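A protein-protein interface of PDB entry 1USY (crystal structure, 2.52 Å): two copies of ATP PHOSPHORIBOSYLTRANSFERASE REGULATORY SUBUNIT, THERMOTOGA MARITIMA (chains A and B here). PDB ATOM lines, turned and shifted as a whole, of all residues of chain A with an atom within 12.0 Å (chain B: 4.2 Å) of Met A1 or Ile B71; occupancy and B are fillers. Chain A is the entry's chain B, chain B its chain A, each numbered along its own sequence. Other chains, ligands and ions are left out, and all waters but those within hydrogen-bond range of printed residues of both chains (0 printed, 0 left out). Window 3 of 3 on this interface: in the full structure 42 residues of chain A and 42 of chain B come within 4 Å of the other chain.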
ATOM      1  N   MET A   1      -7.547  -9.463  -1.791  1.00  0.00           N
ATOM      2  CA  MET A   1      -8.547 -10.534  -2.097  1.00  0.00           C
ATOM      3  C   MET A   1      -9.347 -10.249  -3.370  1.00  0.00           C
ATOM      4  O   MET A   1     -10.412  -9.622  -3.320  1.00  0.00           O
ATOM      5  CB  MET A   1      -9.505 -10.761  -0.940  1.00  0.00           C
ATOM      6  CG  MET A   1     -10.125 -12.143  -1.019  1.00  0.00           C
ATOM      7  SD  MET A   1     -11.629 -12.322  -0.120  1.00  0.00           S
ATOM      8  CE  MET A   1     -12.667 -11.062  -0.821  1.00  0.00           C
ATOM      9  N   ASP A   2      -8.819 -10.754  -4.487  1.00  0.00           N
ATOM     10  CA  ASP A   2      -9.355 -10.541  -5.829  1.00  0.00           C
ATOM     11  C   ASP A   2      -9.448  -9.047  -6.055  1.00  0.00           C
ATOM     12  O   ASP A   2     -10.503  -8.504  -6.368  1.00  0.00           O
ATOM     13  CB  ASP A   2     -10.695 -11.246  -6.011  1.00  0.00           C
ATOM     14  CG  ASP A   2     -10.590 -12.766  -5.850  1.00  0.00           C
ATOM     15  OD1 ASP A   2      -9.960 -13.438  -6.716  1.00  0.00           O
ATOM     16  OD2 ASP A   2     -11.131 -13.373  -4.890  1.00  0.00           O
ATOM     17  N   PHE A   3      -8.304  -8.405  -5.852  1.00  0.00           N
ATOM     18  CA  PHE A   3      -8.161  -6.970  -5.930  1.00  0.00           C
ATOM     19  C   PHE A   3      -7.781  -6.594  -7.350  1.00  0.00           C
ATOM     20  O   PHE A   3      -7.058  -7.320  -7.999  1.00  0.00           O
ATOM     21  CB  PHE A   3      -7.075  -6.503  -4.961  1.00  0.00           C
ATOM     22  CG  PHE A   3      -6.640  -5.087  -5.196  1.00  0.00           C
ATOM     23  CD1 PHE A   3      -7.143  -4.060  -4.403  1.00  0.00           C
ATOM     24  CD2 PHE A   3      -5.752  -4.775  -6.225  1.00  0.00           C
ATOM     25  CE1 PHE A   3      -6.752  -2.752  -4.620  1.00  0.00           C
ATOM     26  CE2 PHE A   3      -5.372  -3.467  -6.443  1.00  0.00           C
ATOM     27  CZ  PHE A   3      -5.875  -2.458  -5.638  1.00  0.00           C
ATOM     28  N   LEU A   4      -8.271  -5.447  -7.807  1.00  0.00           N
ATOM     29  CA  LEU A   4      -7.944  -4.890  -9.119  1.00  0.00           C
ATOM     30  C   LEU A   4      -7.524  -3.447  -8.891  1.00  0.00           C
ATOM     31  O   LEU A   4      -8.147  -2.750  -8.099  1.00  0.00           O
ATOM     32  CB  LEU A   4      -9.169  -4.948 -10.046  1.00  0.00           C
ATOM     33  CG  LEU A   4      -8.987  -4.718 -11.552  1.00  0.00           C
ATOM     34  CD1 LEU A   4      -8.730  -6.012 -12.321  1.00  0.00           C
ATOM     35  CD2 LEU A   4     -10.172  -4.061 -12.162  1.00  0.00           C
ATOM     36  N   ASP A   5      -6.454  -2.994  -9.540  1.00  0.00           N
ATOM     37  CA  ASP A   5      -6.154  -1.566  -9.518  1.00  0.00           C
ATOM     38  C   ASP A   5      -7.127  -0.896 -10.480  1.00  0.00           C
ATOM     39  O   ASP A   5      -6.851  -0.762 -11.664  1.00  0.00           O
ATOM     40  CB  ASP A   5      -4.707  -1.257  -9.884  1.00  0.00           C
ATOM     41  CG  ASP A   5      -4.319   0.183  -9.549  1.00  0.00           C
ATOM     42  OD1 ASP A   5      -3.185   0.592  -9.871  1.00  0.00           O
ATOM     43  OD2 ASP A   5      -5.082   0.991  -8.972  1.00  0.00           O
ATOM     44  N   PHE A   6      -8.277  -0.504  -9.956  1.00  0.00           N
ATOM     45  CA  PHE A   6      -9.345   0.032 -10.782  1.00  0.00           C
ATOM     46  C   PHE A   6      -9.037   1.472 -11.212  1.00  0.00           C
ATOM     47  O   PHE A   6      -9.593   1.940 -12.211  1.00  0.00           O
ATOM     48  CB  PHE A   6     -10.643  -0.037 -10.011  1.00  0.00           C
ATOM     49  CG  PHE A   6     -11.846   0.358 -10.792  1.00  0.00           C
ATOM     50  CD1 PHE A   6     -12.309   1.682 -10.760  1.00  0.00           C
ATOM     51  CD2 PHE A   6     -12.564  -0.603 -11.510  1.00  0.00           C
ATOM     52  CE1 PHE A   6     -13.456   2.060 -11.454  1.00  0.00           C
ATOM     53  CE2 PHE A   6     -13.721  -0.244 -12.217  1.00  0.00           C
ATOM     54  CZ  PHE A   6     -14.162   1.103 -12.191  1.00  0.00           C
ATOM     55  N   PHE A  78     -13.111  -9.832 -18.139  1.00  0.00           N
ATOM     56  CA  PHE A  78     -12.407 -11.065 -18.228  1.00  0.00           C
ATOM     57  C   PHE A  78     -12.553 -11.644 -19.615  1.00  0.00           C
ATOM     58  O   PHE A  78     -13.609 -11.506 -20.219  1.00  0.00           O
ATOM     59  CB  PHE A  78     -12.934 -12.006 -17.173  1.00  0.00           C
ATOM     60  CG  PHE A  78     -12.507 -11.631 -15.789  1.00  0.00           C
ATOM     61  CD1 PHE A  78     -13.404 -11.099 -14.888  1.00  0.00           C
ATOM     62  CD2 PHE A  78     -11.177 -11.771 -15.403  1.00  0.00           C
ATOM     63  CE1 PHE A  78     -12.967 -10.732 -13.593  1.00  0.00           C
ATOM     64  CE2 PHE A  78     -10.749 -11.420 -14.117  1.00  0.00           C
ATOM     65  CZ  PHE A  78     -11.626 -10.905 -13.222  1.00  0.00           C
ATOM     66  N   TYR A  91      -7.959 -10.665 -17.001  1.00  0.00           N
ATOM     67  CA  TYR A  91      -8.705  -9.408 -17.047  1.00  0.00           C
ATOM     68  C   TYR A  91      -8.073  -8.465 -18.075  1.00  0.00           C
ATOM     69  O   TYR A  91      -6.885  -8.128 -17.986  1.00  0.00           O
ATOM     70  CB  TYR A  91      -8.690  -8.737 -15.672  1.00  0.00           C
ATOM     71  CG  TYR A  91      -9.678  -7.573 -15.584  1.00  0.00           C
ATOM     72  CD1 TYR A  91     -10.977  -7.783 -15.090  1.00  0.00           C
ATOM     73  CD2 TYR A  91      -9.288  -6.294 -16.002  1.00  0.00           C
ATOM     74  CE1 TYR A  91     -11.882  -6.710 -15.014  1.00  0.00           C
ATOM     75  CE2 TYR A  91     -10.192  -5.223 -15.926  1.00  0.00           C
ATOM     76  CZ  TYR A  91     -11.486  -5.431 -15.433  1.00  0.00           C
ATOM     77  OH  TYR A  91     -12.354  -4.385 -15.358  1.00  0.00           O
ATOM     78  N   GLU A 271      -4.588  -8.938 -16.065  1.00  0.00           N
ATOM     79  CA  GLU A 271      -4.719 -10.401 -15.995  1.00  0.00           C
ATOM     80  C   GLU A 271      -4.755 -11.029 -14.608  1.00  0.00           C
ATOM     81  O   GLU A 271      -4.876 -10.315 -13.600  1.00  0.00           O
ATOM     82  CB  GLU A 271      -3.661 -11.074 -16.887  1.00  0.00           C
ATOM     83  CG  GLU A 271      -3.983 -10.953 -18.356  1.00  0.00           C
ATOM     84  CD  GLU A 271      -3.616 -12.188 -19.151  1.00  0.00           C
ATOM     85  OE1 GLU A 271      -4.350 -12.515 -20.128  1.00  0.00           O
ATOM     86  OE2 GLU A 271      -2.595 -12.829 -18.812  1.00  0.00           O
ATOM     87  N   GLY A 272      -4.669 -12.364 -14.578  1.00  0.00           N
ATOM     88  CA  GLY A 272      -4.634 -13.110 -13.338  1.00  0.00           C
ATOM     89  C   GLY A 272      -5.773 -14.088 -13.278  1.00  0.00           C
ATOM     90  O   GLY A 272      -6.156 -14.630 -14.300  1.00  0.00           O
ATOM     91  N   LYS A 273      -6.259 -14.346 -12.068  1.00  0.00           N
ATOM     92  CA  LYS A 273      -7.526 -15.062 -11.782  1.00  0.00           C
ATOM     93  C   LYS A 273      -7.750 -16.496 -12.330  1.00  0.00           C
ATOM     94  O   LYS A 273      -7.443 -16.804 -13.477  1.00  0.00           O
ATOM     95  CB  LYS A 273      -8.726 -14.139 -12.048  1.00  0.00           C
ATOM     96  CG  LYS A 273      -8.557 -12.712 -11.439  1.00  0.00           C
ATOM     97  CD  LYS A 273      -8.837 -12.659  -9.933  1.00  0.00           C
ATOM     98  CE  LYS A 273      -7.611 -12.218  -9.142  1.00  0.00           C
ATOM     99  NZ  LYS A 273      -7.146 -13.272  -8.180  1.00  0.00           N
ATOM    100  N   THR A 274      -8.288 -17.368 -11.486  1.00  0.00           N
ATOM    101  CA  THR A 274      -8.556 -18.756 -11.873  1.00  0.00           C
ATOM    102  C   THR A 274     -10.044 -18.981 -11.767  1.00  0.00           C
ATOM    103  O   THR A 274     -10.670 -18.530 -10.801  1.00  0.00           O
ATOM    104  CB  THR A 274      -7.815 -19.734 -10.942  1.00  0.00           C
ATOM    105  OG1 THR A 274      -6.402 -19.502 -11.042  1.00  0.00           O
ATOM    106  CG2 THR A 274      -7.973 -21.177 -11.420  1.00  0.00           C
ATOM    107  N   PHE B  24     -13.434  -5.424  -5.848  1.00  0.00           N
ATOM    108  CA  PHE B  24     -13.520  -6.851  -5.912  1.00  0.00           C
ATOM    109  C   PHE B  24     -13.968  -7.331  -7.285  1.00  0.00           C
ATOM    110  O   PHE B  24     -15.117  -7.225  -7.607  1.00  0.00           O
ATOM    111  CB  PHE B  24     -14.473  -7.345  -4.828  1.00  0.00           C
ATOM    112  CG  PHE B  24     -14.584  -8.846  -4.761  1.00  0.00           C
ATOM    113  CD1 PHE B  24     -13.635  -9.588  -4.057  1.00  0.00           C
ATOM    114  CD2 PHE B  24     -15.628  -9.521  -5.413  1.00  0.00           C
ATOM    115  CE1 PHE B  24     -13.746 -10.960  -3.976  1.00  0.00           C
ATOM    116  CE2 PHE B  24     -15.753 -10.918  -5.328  1.00  0.00           C
ATOM    117  CZ  PHE B  24     -14.809 -11.637  -4.611  1.00  0.00           C
ATOM    118  N   HIS B  61     -15.296 -16.906  -1.135  1.00  0.00           N
ATOM    119  CA  HIS B  61     -14.034 -16.443  -1.707  1.00  0.00           C
ATOM    120  C   HIS B  61     -13.155 -15.948  -0.559  1.00  0.00           C
ATOM    121  O   HIS B  61     -11.931 -15.997  -0.597  1.00  0.00           O
ATOM    122  CB  HIS B  61     -14.302 -15.261  -2.620  1.00  0.00           C
ATOM    123  CG  HIS B  61     -14.082 -15.554  -4.069  1.00  0.00           C
ATOM    124  ND1 HIS B  61     -12.868 -15.354  -4.686  1.00  0.00           N
ATOM    125  CD2 HIS B  61     -14.923 -16.017  -5.028  1.00  0.00           C
ATOM    126  CE1 HIS B  61     -12.960 -15.713  -5.955  1.00  0.00           C
ATOM    127  NE2 HIS B  61     -14.202 -16.097  -6.192  1.00  0.00           N
ATOM    128  N   ARG B  62     -13.819 -15.420   0.451  1.00  0.00           N
ATOM    129  CA  ARG B  62     -13.187 -14.985   1.676  1.00  0.00           C
ATOM    130  C   ARG B  62     -12.863 -16.202   2.538  1.00  0.00           C
ATOM    131  O   ARG B  62     -11.876 -16.181   3.284  1.00  0.00           O
ATOM    132  CB  ARG B  62     -14.117 -13.983   2.374  1.00  0.00           C
ATOM    133  CG  ARG B  62     -13.873 -13.768   3.829  1.00  0.00           C
ATOM    134  CD  ARG B  62     -15.005 -13.081   4.497  1.00  0.00           C
ATOM    135  NE  ARG B  62     -15.430 -13.814   5.680  1.00  0.00           N
ATOM    136  CZ  ARG B  62     -14.901 -13.625   6.878  1.00  0.00           C
ATOM    137  NH1 ARG B  62     -13.945 -12.720   7.033  1.00  0.00           N
ATOM    138  NH2 ARG B  62     -15.322 -14.331   7.922  1.00  0.00           N
ATOM    139  N   TYR B  65      -9.360 -18.238   3.109  1.00  0.00           N
ATOM    140  CA  TYR B  65      -8.329 -17.537   3.904  1.00  0.00           C
ATOM    141  C   TYR B  65      -8.247 -17.950   5.378  1.00  0.00           C
ATOM    142  O   TYR B  65      -9.223 -17.832   6.118  1.00  0.00           O
ATOM    143  CB  TYR B  65      -8.493 -16.020   3.784  1.00  0.00           C
ATOM    144  CG  TYR B  65      -8.094 -15.472   2.437  1.00  0.00           C
ATOM    145  CD1 TYR B  65      -6.912 -14.771   2.282  1.00  0.00           C
ATOM    146  CD2 TYR B  65      -8.911 -15.640   1.323  1.00  0.00           C
ATOM    147  CE1 TYR B  65      -6.545 -14.259   1.046  1.00  0.00           C
ATOM    148  CE2 TYR B  65      -8.554 -15.144   0.088  1.00  0.00           C
ATOM    149  CZ  TYR B  65      -7.377 -14.448  -0.044  1.00  0.00           C
ATOM    150  OH  TYR B  65      -6.999 -13.950  -1.266  1.00  0.00           O
ATOM    151  N   SER B  69      -9.859 -13.183   7.464  1.00  0.00           N
ATOM    152  CA  SER B  69      -9.864 -11.915   6.702  1.00  0.00           C
ATOM    153  C   SER B  69     -10.856 -10.900   7.230  1.00  0.00           C
ATOM    154  O   SER B  69     -11.987 -11.223   7.562  1.00  0.00           O
ATOM    155  CB  SER B  69     -10.206 -12.115   5.221  1.00  0.00           C
ATOM    156  OG  SER B  69      -9.194 -12.782   4.511  1.00  0.00           O
ATOM    157  N   GLN B  70     -10.431  -9.653   7.275  1.00  0.00           N
ATOM    158  CA  GLN B  70     -11.354  -8.556   7.493  1.00  0.00           C
ATOM    159  C   GLN B  70     -11.616  -7.970   6.116  1.00  0.00           C
ATOM    160  O   GLN B  70     -10.720  -7.379   5.523  1.00  0.00           O
ATOM    161  CB  GLN B  70     -10.708  -7.530   8.408  1.00  0.00           C
ATOM    162  CG  GLN B  70     -11.553  -6.305   8.683  1.00  0.00           C
ATOM    163  CD  GLN B  70     -11.731  -6.031  10.177  1.00  0.00           C
ATOM    164  OE1 GLN B  70     -12.506  -5.136  10.545  1.00  0.00           O
ATOM    165  NE2 GLN B  70     -11.020  -6.791  11.041  1.00  0.00           N
ATOM    166  N   ILE B  71     -12.836  -8.145   5.607  1.00  0.00           N
ATOM    167  CA  ILE B  71     -13.164  -7.777   4.230  1.00  0.00           C
ATOM    168  C   ILE B  71     -14.071  -6.554   4.110  1.00  0.00           C
ATOM    169  O   ILE B  71     -15.068  -6.468   4.812  1.00  0.00           O
ATOM    170  CB  ILE B  71     -13.724  -8.997   3.492  1.00  0.00           C
ATOM    171  CG1 ILE B  71     -12.716  -9.425   2.432  1.00  0.00           C
ATOM    172  CG2 ILE B  71     -15.074  -8.717   2.852  1.00  0.00           C
ATOM    173  CD1 ILE B  71     -12.362 -10.905   2.474  1.00  0.00           C
ATOM    174  N   LYS B  72     -13.676  -5.609   3.247  1.00  0.00           N
ATOM    175  CA  LYS B  72     -14.383  -4.348   2.964  1.00  0.00           C
ATOM    176  C   LYS B  72     -14.214  -3.991   1.477  1.00  0.00           C
ATOM    177  O   LYS B  72     -13.211  -3.461   1.068  1.00  0.00           O
ATOM    178  CB  LYS B  72     -13.825  -3.205   3.802  1.00  0.00           C
ATOM    179  CG  LYS B  72     -14.763  -1.992   3.992  1.00  0.00           C
ATOM    180  CD  LYS B  72     -14.113  -0.943   4.919  1.00  0.00           C
ATOM    181  CE  LYS B  72     -15.145   0.074   5.432  1.00  0.00           C
ATOM    182  NZ  LYS B  72     -14.792   0.596   6.807  1.00  0.00           N
ATOM    183  N   GLU B  96     -19.766  -4.832   0.315  1.00  0.00           N
ATOM    184  CA  GLU B  96     -19.777  -5.978   1.212  1.00  0.00           C
ATOM    185  C   GLU B  96     -18.760  -5.685   2.306  1.00  0.00           C
ATOM    186  O   GLU B  96     -17.614  -5.328   2.047  1.00  0.00           O
ATOM    187  CB  GLU B  96     -19.413  -7.252   0.431  1.00  0.00           C
ATOM    188  CG  GLU B  96     -20.377  -8.454   0.439  1.00  0.00           C
ATOM    189  CD  GLU B  96     -21.870  -8.163   0.252  1.00  0.00           C
ATOM    190  OE1 GLU B  96     -22.586  -8.188   1.271  1.00  0.00           O
ATOM    191  OE2 GLU B  96     -22.354  -7.979  -0.888  1.00  0.00           O
ATOM    192  N   LYS B  97     -19.188  -5.759   3.533  1.00  0.00           N
ATOM    193  CA  LYS B  97     -18.279  -5.638   4.665  1.00  0.00           C
ATOM    194  C   LYS B  97     -18.579  -6.730   5.679  1.00  0.00           C
ATOM    195  O   LYS B  97     -19.710  -6.866   6.109  1.00  0.00           O
ATOM    196  CB  LYS B  97     -18.355  -4.241   5.330  1.00  0.00           C
ATOM    197  CG  LYS B  97     -17.405  -4.157   6.539  1.00  0.00           C
ATOM    198  CD  LYS B  97     -17.047  -2.780   6.947  1.00  0.00           C
ATOM    199  CE  LYS B  97     -15.835  -2.785   7.865  1.00  0.00           C
ATOM    200  NZ  LYS B  97     -16.078  -3.492   9.128  1.00  0.00           N
ATOM    201  N   VAL B  98     -17.560  -7.498   6.025  1.00  0.00           N
ATOM    202  CA  VAL B  98     -17.621  -8.561   7.029  1.00  0.00           C
ATOM    203  C   VAL B  98     -16.354  -8.399   7.836  1.00  0.00           C
ATOM    204  O   VAL B  98     -15.307  -8.718   7.321  1.00  0.00           O
ATOM    205  CB  VAL B  98     -17.465  -9.950   6.387  1.00  0.00           C
ATOM    206  CG1 VAL B  98     -17.199 -10.980   7.451  1.00  0.00           C
ATOM    207  CG2 VAL B  98     -18.676 -10.341   5.579  1.00  0.00           C
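A ring nitrogen (ND1) of His B61 lies within hydrogen-bond range of the side-chain carboxylate (OD2) of Asp A2 (2.6 Å).
The side-chain sulfur of Met A1 sits close to the backbone carbonyl oxygen of His B61 (3.7 Å).
NH1 of Arg B62 lies within hydrogen-bond range of O of Ser B69 (2.5 Å).
The backbone NH (N) of Val B98 is in hydrogen-bond range of the backbone carbonyl oxygen (O) of Ile B71.
The side-chain carboxylate of Asp A2 lies within salt-bridge range of the side-chain amino group of Lys A273 (3.2 Å).
Among the printed residues, pairs that only touch across the chains: Met A1 with Phe B24 (3.3 Å), Met A1 with Arg B62 (3.6 Å), Met A1 with Tyr B65 (3.6 Å), Met A1 with Ile B71 (3.0 Å) and Asp A2 with Phe B24 (3.5 Å).
Met A1 touches just these residues of chain B: Phe B24, His B61, Arg B62, Tyr B65 and Ile B71.
Printed residues of chain B within 4 Å of Asp A2: Phe B24 and His B61.
Leu A4 touches none of the printed residues of chain B.
Of the printed residues of chain A, Phe B24 touches Met A1 (3.3 Å) and Asp A2 (3.5 Å).
Of chain A, only Met A1 and Asp A2 come within 4 Å of His B61.
Of chain A, only Met A1 (3.6 Å) comes within 4 Å of Arg B62.
Printed residues of chain A within 4 Å of Tyr B65: Met A1 (3.6 Å).
Ser B69 touches none of the printed residues of chain A.
Printed residues of chain A within 4 Å of Ile B71: Met A1 (3.0 Å).
No residue of chain A comes within 4 Å of Lys B97.
The nearest residue of chain A that does not touch Ile B71 is Asp A2 (7.8 Å).
The nearest printed residue of chain A that does not touch Tyr B65 is Asp A2 (4.9 Å).
Printed residues of chain A that touch a printed residue of chain B: Met A1 and Asp A2.
No position is printed for both chains.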
